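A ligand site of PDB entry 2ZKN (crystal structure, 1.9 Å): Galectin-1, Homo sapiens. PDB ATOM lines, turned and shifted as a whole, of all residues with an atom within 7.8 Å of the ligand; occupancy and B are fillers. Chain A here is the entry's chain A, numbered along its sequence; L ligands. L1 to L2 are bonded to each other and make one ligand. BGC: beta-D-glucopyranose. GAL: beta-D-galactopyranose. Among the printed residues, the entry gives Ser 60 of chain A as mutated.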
ATOM      1  N   SER A  29     -10.903 -15.396  22.554  1.00  0.00           N
ATOM      2  CA  SER A  29      -9.708 -16.084  22.073  1.00  0.00           C
ATOM      3  C   SER A  29      -9.790 -16.321  20.564  1.00  0.00           C
ATOM      4  O   SER A  29     -10.832 -16.115  19.964  1.00  0.00           O
ATOM      5  CB  SER A  29      -9.549 -17.430  22.766  1.00  0.00           C
ATOM      6  OG  SER A  29     -10.447 -18.393  22.216  1.00  0.00           O
ATOM      7  N   PHE A  30      -8.681 -16.743  19.974  1.00  0.00           N
ATOM      8  CA  PHE A  30      -8.675 -17.054  18.557  1.00  0.00           C
ATOM      9  C   PHE A  30      -7.806 -18.286  18.319  1.00  0.00           C
ATOM     10  O   PHE A  30      -6.982 -18.651  19.175  1.00  0.00           O
ATOM     11  CB  PHE A  30      -8.254 -15.844  17.695  1.00  0.00           C
ATOM     12  CG  PHE A  30      -6.781 -15.521  17.719  1.00  0.00           C
ATOM     13  CD1 PHE A  30      -5.901 -16.122  16.823  1.00  0.00           C
ATOM     14  CD2 PHE A  30      -6.286 -14.540  18.588  1.00  0.00           C
ATOM     15  CE1 PHE A  30      -4.557 -15.755  16.781  1.00  0.00           C
ATOM     16  CE2 PHE A  30      -4.939 -14.167  18.553  1.00  0.00           C
ATOM     17  CZ  PHE A  30      -4.070 -14.774  17.639  1.00  0.00           C
ATOM     18  N   VAL A  31      -8.012 -18.935  17.189  1.00  0.00           N
ATOM     19  CA  VAL A  31      -7.291 -20.159  16.888  1.00  0.00           C
ATOM     20  C   VAL A  31      -6.721 -20.256  15.490  1.00  0.00           C
ATOM     21  O   VAL A  31      -7.314 -19.781  14.520  1.00  0.00           O
ATOM     22  CB  VAL A  31      -8.226 -21.392  17.097  1.00  0.00           C
ATOM     23  CG1 VAL A  31      -7.545 -22.672  16.642  1.00  0.00           C
ATOM     24  CG2 VAL A  31      -8.623 -21.494  18.559  1.00  0.00           C
ATOM     25  N   ASN A  33      -5.014 -23.448  13.450  1.00  0.00           N
ATOM     26  CA  ASN A  33      -4.673 -24.875  13.485  1.00  0.00           C
ATOM     27  C   ASN A  33      -3.835 -25.289  12.285  1.00  0.00           C
ATOM     28  O   ASN A  33      -4.068 -24.821  11.170  1.00  0.00           O
ATOM     29  CB  ASN A  33      -5.930 -25.742  13.507  1.00  0.00           C
ATOM     30  CG  ASN A  33      -6.722 -25.593  14.792  1.00  0.00           C
ATOM     31  OD1 ASN A  33      -6.151 -25.451  15.871  1.00  0.00           O
ATOM     32  ND2 ASN A  33      -8.045 -25.661  14.689  1.00  0.00           N
ATOM     33  N   HIS A  44      -2.263 -26.590  17.493  1.00  0.00           N
ATOM     34  CA  HIS A  44      -3.497 -25.869  17.754  1.00  0.00           C
ATOM     35  C   HIS A  44      -2.933 -24.676  18.527  1.00  0.00           C
ATOM     36  O   HIS A  44      -2.577 -24.805  19.694  1.00  0.00           O
ATOM     37  CB  HIS A  44      -4.423 -26.721  18.643  1.00  0.00           C
ATOM     38  CG  HIS A  44      -5.574 -25.967  19.233  1.00  0.00           C
ATOM     39  ND1 HIS A  44      -6.612 -25.463  18.482  1.00  0.00           N
ATOM     40  CD2 HIS A  44      -5.874 -25.676  20.530  1.00  0.00           C
ATOM     41  CE1 HIS A  44      -7.505 -24.900  19.284  1.00  0.00           C
ATOM     42  NE2 HIS A  44      -7.078 -25.017  20.523  1.00  0.00           N
ATOM     43  N   PHE A  45      -2.819 -23.539  17.848  1.00  0.00           N
ATOM     44  CA  PHE A  45      -2.286 -22.300  18.432  1.00  0.00           C
ATOM     45  C   PHE A  45      -3.491 -21.499  18.907  1.00  0.00           C
ATOM     46  O   PHE A  45      -4.234 -20.957  18.098  1.00  0.00           O
ATOM     47  CB  PHE A  45      -1.504 -21.534  17.371  1.00  0.00           C
ATOM     48  CG  PHE A  45      -0.920 -20.246  17.855  1.00  0.00           C
ATOM     49  CD1 PHE A  45       0.150 -20.241  18.751  1.00  0.00           C
ATOM     50  CD2 PHE A  45      -1.440 -19.028  17.420  1.00  0.00           C
ATOM     51  CE1 PHE A  45       0.683 -19.046  19.205  1.00  0.00           C
ATOM     52  CE2 PHE A  45      -0.907 -17.832  17.874  1.00  0.00           C
ATOM     53  CZ  PHE A  45       0.163 -17.841  18.770  1.00  0.00           C
ATOM     54  N   ASN A  46      -3.638 -21.397  20.221  1.00  0.00           N
ATOM     55  CA  ASN A  46      -4.811 -20.756  20.804  1.00  0.00           C
ATOM     56  C   ASN A  46      -4.581 -19.640  21.828  1.00  0.00           C
ATOM     57  O   ASN A  46      -4.603 -19.898  23.028  1.00  0.00           O
ATOM     58  CB  ASN A  46      -5.675 -21.861  21.421  1.00  0.00           C
ATOM     59  CG  ASN A  46      -6.993 -21.350  21.992  1.00  0.00           C
ATOM     60  OD1 ASN A  46      -7.617 -22.037  22.807  1.00  0.00           O
ATOM     61  ND2 ASN A  46      -7.427 -20.179  21.558  1.00  0.00           N
ATOM     62  N   ARG A  48      -5.516 -17.080  24.296  1.00  0.00           N
ATOM     63  CA  ARG A  48      -6.749 -16.854  25.045  1.00  0.00           C
ATOM     64  C   ARG A  48      -6.714 -15.535  25.809  1.00  0.00           C
ATOM     65  O   ARG A  48      -5.850 -15.319  26.664  1.00  0.00           O
ATOM     66  CB  ARG A  48      -6.995 -18.010  26.014  1.00  0.00           C
ATOM     67  CG  ARG A  48      -7.163 -19.364  25.337  1.00  0.00           C
ATOM     68  CD  ARG A  48      -7.258 -20.511  26.335  1.00  0.00           C
ATOM     69  NE  ARG A  48      -7.489 -21.788  25.660  1.00  0.00           N
ATOM     70  CZ  ARG A  48      -7.568 -22.965  26.280  1.00  0.00           C
ATOM     71  NH1 ARG A  48      -7.442 -23.028  27.594  1.00  0.00           N
ATOM     72  NH2 ARG A  48      -7.785 -24.070  25.587  1.00  0.00           N
ATOM     73  N   ALA A  51     -10.642 -17.133  28.447  1.00  0.00           N
ATOM     74  CA  ALA A  51     -11.364 -18.362  28.141  1.00  0.00           C
ATOM     75  C   ALA A  51     -10.775 -19.573  28.845  1.00  0.00           C
ATOM     76  O   ALA A  51      -9.546 -19.706  28.951  1.00  0.00           O
ATOM     77  CB  ALA A  51     -11.373 -18.584  26.636  1.00  0.00           C
ATOM     78  N   HIS A  52     -11.647 -20.445  29.341  1.00  0.00           N
ATOM     79  CA  HIS A  52     -11.232 -21.665  30.015  1.00  0.00           C
ATOM     80  C   HIS A  52     -10.336 -21.433  31.231  1.00  0.00           C
ATOM     81  O   HIS A  52      -9.483 -22.256  31.547  1.00  0.00           O
ATOM     82  CB  HIS A  52     -10.531 -22.589  29.019  1.00  0.00           C
ATOM     83  CG  HIS A  52     -11.353 -22.905  27.819  1.00  0.00           C
ATOM     84  ND1 HIS A  52     -12.541 -23.604  27.887  1.00  0.00           N
ATOM     85  CD2 HIS A  52     -11.189 -22.582  26.511  1.00  0.00           C
ATOM     86  CE1 HIS A  52     -13.068 -23.695  26.679  1.00  0.00           C
ATOM     87  NE2 HIS A  52     -12.274 -23.081  25.824  1.00  0.00           N
ATOM     88  N   GLY A  53     -10.532 -20.297  31.901  1.00  0.00           N
ATOM     89  CA  GLY A  53      -9.721 -20.000  33.066  1.00  0.00           C
ATOM     90  C   GLY A  53      -8.435 -19.271  32.731  1.00  0.00           C
ATOM     91  O   GLY A  53      -7.749 -18.777  33.631  1.00  0.00           O
ATOM     92  N   ASP A  54      -8.096 -19.201  31.449  1.00  0.00           N
ATOM     93  CA  ASP A  54      -6.884 -18.504  31.018  1.00  0.00           C
ATOM     94  C   ASP A  54      -7.132 -17.027  30.745  1.00  0.00           C
ATOM     95  O   ASP A  54      -8.109 -16.662  30.093  1.00  0.00           O
ATOM     96  CB  ASP A  54      -6.309 -19.161  29.761  1.00  0.00           C
ATOM     97  CG  ASP A  54      -5.659 -20.496  30.037  1.00  0.00           C
ATOM     98  OD1 ASP A  54      -6.178 -21.519  29.547  1.00  0.00           O
ATOM     99  OD2 ASP A  54      -4.620 -20.516  30.740  1.00  0.00           O
ATOM    100  N   VAL A  59      -1.992 -20.757  24.555  1.00  0.00           N
ATOM    101  CA  VAL A  59      -2.100 -22.190  24.819  1.00  0.00           C
ATOM    102  C   VAL A  59      -1.898 -22.921  23.500  1.00  0.00           C
ATOM    103  O   VAL A  59      -2.549 -22.594  22.503  1.00  0.00           O
ATOM    104  CB  VAL A  59      -3.481 -22.566  25.402  1.00  0.00           C
ATOM    105  CG1 VAL A  59      -3.554 -24.068  25.640  1.00  0.00           C
ATOM    106  CG2 VAL A  59      -3.723 -21.820  26.698  1.00  0.00           C
ATOM    107  N   SER A  60      -0.987 -23.888  23.492  1.00  0.00           N
ATOM    108  CA  SER A  60      -0.723 -24.682  22.299  1.00  0.00           C
ATOM    109  C   SER A  60      -0.959 -26.156  22.620  1.00  0.00           C
ATOM    110  O   SER A  60      -0.781 -26.591  23.765  1.00  0.00           O
ATOM    111  CB  SER A  60       0.724 -24.494  21.818  1.00  0.00           C
ATOM    112  OG  SER A  60       0.958 -23.169  21.355  1.00  0.00           O
ATOM    113  N   ASN A  61      -1.392 -26.923  21.627  1.00  0.00           N
ATOM    114  CA  ASN A  61      -1.621 -28.342  21.852  1.00  0.00           C
ATOM    115  C   ASN A  61      -1.660 -29.070  20.532  1.00  0.00           C
ATOM    116  O   ASN A  61      -1.680 -28.452  19.461  1.00  0.00           O
ATOM    117  CB  ASN A  61      -2.937 -28.571  22.602  1.00  0.00           C
ATOM    118  CG  ASN A  61      -2.972 -29.916  23.347  1.00  0.00           C
ATOM    119  OD1 ASN A  61      -2.091 -30.762  23.178  1.00  0.00           O
ATOM    120  ND2 ASN A  61      -3.989 -30.100  24.173  1.00  0.00           N
ATOM    121  N   SER A  62      -1.646 -30.385  20.609  1.00  0.00           N
ATOM    122  CA  SER A  62      -1.708 -31.242  19.443  1.00  0.00           C
ATOM    123  C   SER A  62      -3.064 -31.937  19.529  1.00  0.00           C
ATOM    124  O   SER A  62      -3.744 -31.865  20.559  1.00  0.00           O
ATOM    125  CB  SER A  62      -0.589 -32.287  19.489  1.00  0.00           C
ATOM    126  OG  SER A  62      -0.673 -33.063  20.681  1.00  0.00           O
ATOM    127  N   LYS A  63      -3.468 -32.579  18.445  1.00  0.00           N
ATOM    128  CA  LYS A  63      -4.733 -33.301  18.411  1.00  0.00           C
ATOM    129  C   LYS A  63      -4.469 -34.531  17.563  1.00  0.00           C
ATOM    130  O   LYS A  63      -4.130 -34.417  16.377  1.00  0.00           O
ATOM    131  CB  LYS A  63      -5.831 -32.423  17.800  1.00  0.00           C
ATOM    132  CG  LYS A  63      -7.239 -32.950  18.038  1.00  0.00           C
ATOM    133  CD  LYS A  63      -8.262 -31.923  17.572  1.00  0.00           C
ATOM    134  CE  LYS A  63      -9.642 -32.193  18.167  1.00  0.00           C
ATOM    135  NZ  LYS A  63     -10.615 -31.135  17.796  1.00  0.00           N
ATOM    136  N   TRP A  68      -7.192 -34.420  22.210  1.00  0.00           N
ATOM    137  CA  TRP A  68      -6.274 -33.348  22.600  1.00  0.00           C
ATOM    138  C   TRP A  68      -5.064 -33.906  23.353  1.00  0.00           C
ATOM    139  O   TRP A  68      -5.208 -34.805  24.189  1.00  0.00           O
ATOM    140  CB  TRP A  68      -6.990 -32.334  23.490  1.00  0.00           C
ATOM    141  CG  TRP A  68      -7.952 -31.460  22.756  1.00  0.00           C
ATOM    142  CD1 TRP A  68      -9.287 -31.315  23.017  1.00  0.00           C
ATOM    143  CD2 TRP A  68      -7.657 -30.594  21.657  1.00  0.00           C
ATOM    144  NE1 TRP A  68      -9.837 -30.398  22.148  1.00  0.00           N
ATOM    145  CE2 TRP A  68      -8.861 -29.937  21.303  1.00  0.00           C
ATOM    146  CE3 TRP A  68      -6.495 -30.292  20.935  1.00  0.00           C
ATOM    147  CZ2 TRP A  68      -8.936 -29.010  20.264  1.00  0.00           C
ATOM    148  CZ3 TRP A  68      -6.570 -29.365  19.897  1.00  0.00           C
ATOM    149  CH2 TRP A  68      -7.787 -28.732  19.576  1.00  0.00           C
ATOM    150  N   GLY A  69      -3.894 -33.372  23.044  1.00  0.00           N
ATOM    151  CA  GLY A  69      -2.683 -33.811  23.700  1.00  0.00           C
ATOM    152  C   GLY A  69      -2.464 -33.036  24.988  1.00  0.00           C
ATOM    153  O   GLY A  69      -3.418 -32.525  25.565  1.00  0.00           O
ATOM    154  N   THR A  70      -1.210 -32.931  25.427  1.00  0.00           N
ATOM    155  CA  THR A  70      -0.902 -32.186  26.647  1.00  0.00           C
ATOM    156  C   THR A  70      -0.602 -30.742  26.257  1.00  0.00           C
ATOM    157  O   THR A  70       0.247 -30.481  25.402  1.00  0.00           O
ATOM    158  CB  THR A  70       0.314 -32.791  27.370  1.00  0.00           C
ATOM    159  OG1 THR A  70       0.059 -34.185  27.631  1.00  0.00           O
ATOM    160  CG2 THR A  70       0.570 -32.081  28.690  1.00  0.00           C
ATOM    161  N   GLU A  71      -1.304 -29.805  26.889  1.00  0.00           N
ATOM    162  CA  GLU A  71      -1.125 -28.390  26.586  1.00  0.00           C
ATOM    163  C   GLU A  71       0.203 -27.787  27.015  1.00  0.00           C
ATOM    164  O   GLU A  71       0.863 -28.273  27.940  1.00  0.00           O
ATOM    165  CB  GLU A  71      -2.254 -27.568  27.233  1.00  0.00           C
ATOM    166  CG  GLU A  71      -3.657 -28.041  26.884  1.00  0.00           C
ATOM    167  CD  GLU A  71      -4.731 -27.251  27.612  1.00  0.00           C
ATOM    168  OE1 GLU A  71      -4.506 -26.843  28.770  1.00  0.00           O
ATOM    169  OE2 GLU A  71      -5.819 -27.040  27.034  1.00  0.00           O
ATOM    170  N   GLN A  72       0.602 -26.735  26.305  1.00  0.00           N
ATOM    171  CA  GLN A  72       1.822 -25.992  26.582  1.00  0.00           C
ATOM    172  C   GLN A  72       1.404 -24.530  26.651  1.00  0.00           C
ATOM    173  O   GLN A  72       0.590 -24.074  25.835  1.00  0.00           O
ATOM    174  CB  GLN A  72       2.854 -26.188  25.476  1.00  0.00           C
ATOM    175  CG  GLN A  72       4.138 -25.375  25.654  1.00  0.00           C
ATOM    176  CD  GLN A  72       5.175 -25.651  24.584  1.00  0.00           C
ATOM    177  OE1 GLN A  72       5.687 -26.768  24.469  1.00  0.00           O
ATOM    178  NE2 GLN A  72       5.487 -24.637  23.777  1.00  0.00           N
ATOM    179  N   ARG A  73       1.936 -23.802  27.628  1.00  0.00           N
ATOM    180  CA  ARG A  73       1.598 -22.387  27.795  1.00  0.00           C
ATOM    181  C   ARG A  73       2.854 -21.521  27.790  1.00  0.00           C
ATOM    182  O   ARG A  73       3.904 -21.961  28.273  1.00  0.00           O
ATOM    183  CB  ARG A  73       0.824 -22.176  29.113  1.00  0.00           C
ATOM    184  CG  ARG A  73      -0.641 -22.630  29.035  1.00  0.00           C
ATOM    185  CD  ARG A  73      -1.373 -22.505  30.373  1.00  0.00           C
ATOM    186  NE  ARG A  73      -2.814 -22.699  30.206  1.00  0.00           N
ATOM    187  CZ  ARG A  73      -3.390 -23.869  29.909  1.00  0.00           C
ATOM    188  NH1 ARG A  73      -2.653 -24.959  29.755  1.00  0.00           N
ATOM    189  NH2 ARG A  73      -4.708 -23.926  29.742  1.00  0.00           N
HETATM  190  C2  BGC L   1      -8.174 -27.158  30.054  1.00  0.00           C
HETATM  191  C3  BGC L   1      -8.720 -26.393  28.853  1.00  0.00           C
HETATM  192  C4  BGC L   1      -9.491 -27.332  27.914  1.00  0.00           C
HETATM  193  C5  BGC L   1     -10.562 -28.097  28.716  1.00  0.00           C
HETATM  194  C6  BGC L   1     -11.332 -29.106  27.884  1.00  0.00           C
HETATM  195  C1  BGC L   1      -9.295 -27.939  30.744  1.00  0.00           C
HETATM  196  O1  BGC L   1      -8.773 -28.715  31.764  1.00  0.00           O
HETATM  197  O2  BGC L   1      -7.586 -26.241  30.968  1.00  0.00           O
HETATM  198  O3  BGC L   1      -7.657 -25.789  28.151  1.00  0.00           O
HETATM  199  O4  BGC L   1     -10.124 -26.536  26.891  1.00  0.00           O
HETATM  200  O5  BGC L   1      -9.949 -28.812  29.807  1.00  0.00           O
HETATM  201  O6  BGC L   1     -10.490 -29.746  26.926  1.00  0.00           O
HETATM  202  C1  GAL L   2      -9.956 -26.964  25.582  1.00  0.00           C
HETATM  203  C2  GAL L   2     -10.794 -26.071  24.657  1.00  0.00           C
HETATM  204  C3  GAL L   2     -10.569 -26.468  23.201  1.00  0.00           C
HETATM  205  C4  GAL L   2      -9.067 -26.458  22.879  1.00  0.00           C
HETATM  206  C5  GAL L   2      -8.306 -27.315  23.891  1.00  0.00           C
HETATM  207  C6  GAL L   2      -6.797 -27.263  23.693  1.00  0.00           C
HETATM  208  O2  GAL L   2     -12.179 -26.206  24.981  1.00  0.00           O
HETATM  209  O3  GAL L   2     -11.238 -25.562  22.351  1.00  0.00           O
HETATM  210  O4  GAL L   2      -8.592 -25.121  22.928  1.00  0.00           O
HETATM  211  O5  GAL L   2      -8.570 -26.856  25.239  1.00  0.00           O
HETATM  212  O6  GAL L   2      -6.141 -28.164  24.577  1.00  0.00           O
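The side-chain carboxylate (OE2) of Glu 71 sits at hydrogen-bond distance from an oxygen (O3) of BGC L1 (2.5 Å).
OD1 of Asn 46 is in hydrogen-bond range of O4 of GAL L2, 3.2 Å away.
An oxygen (O2) of GAL L2 sits close to a ring nitrogen (NE2) of His 52, 3.2 Å away.
NE2 of His 44 lies within hydrogen-bond range of O4 of GAL L2 (2.8 Å).
The side-chain amide nitrogen (ND2) of Asn 61 sits at hydrogen-bond distance from an oxygen (O6) of GAL L2.
An oxygen (O3) of BGC L1 lies within hydrogen-bond range of the guanidinium group of Arg 48.
A ring nitrogen (ND1) of His 44 sits at hydrogen-bond distance from the side-chain amide oxygen of Asn 33.
NH2 of Arg 48 lies within salt-bridge range of OE2 of Glu 71, 3.8 Å away.
NH1 of Arg 48 lies within salt-bridge range of OD1 of Asp 54 (2.8 Å).
The side-chain amide oxygen (OD1) of Asn 46 sits at hydrogen-bond distance from the guanidinium group (NE) of Arg 48.
The side-chain carboxylate (OE1) of Glu 71 lies within salt-bridge range of the guanidinium group (NH1) of Arg 73, at 2.8 Å.
NH2 of Arg 73 lies within salt-bridge range of OD1 of Asp 54, 2.8 Å away.
N of His 44 sits at hydrogen-bond distance from O of Asn 61, at 2.8 Å.
The side-chain amide nitrogen (ND2) of Asn 46 is in hydrogen-bond range of the backbone carbonyl oxygen (O) of Phe 30 (2.9 Å).
Trp 68 touches the ligand.
Arg 73 touches the ligand.
Hydrophobic or aromatic side chains within 4 Å of the ligand: His 44, His 52 and Trp 68.
Within 4 Å of the ligand: His 44, Asn 46, Arg 48, His 52, Asn 61, Trp 68, Glu 71 and Arg 73.
The nearest printed residue that does not touch the ligand is Asp 54 (4.7 Å).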
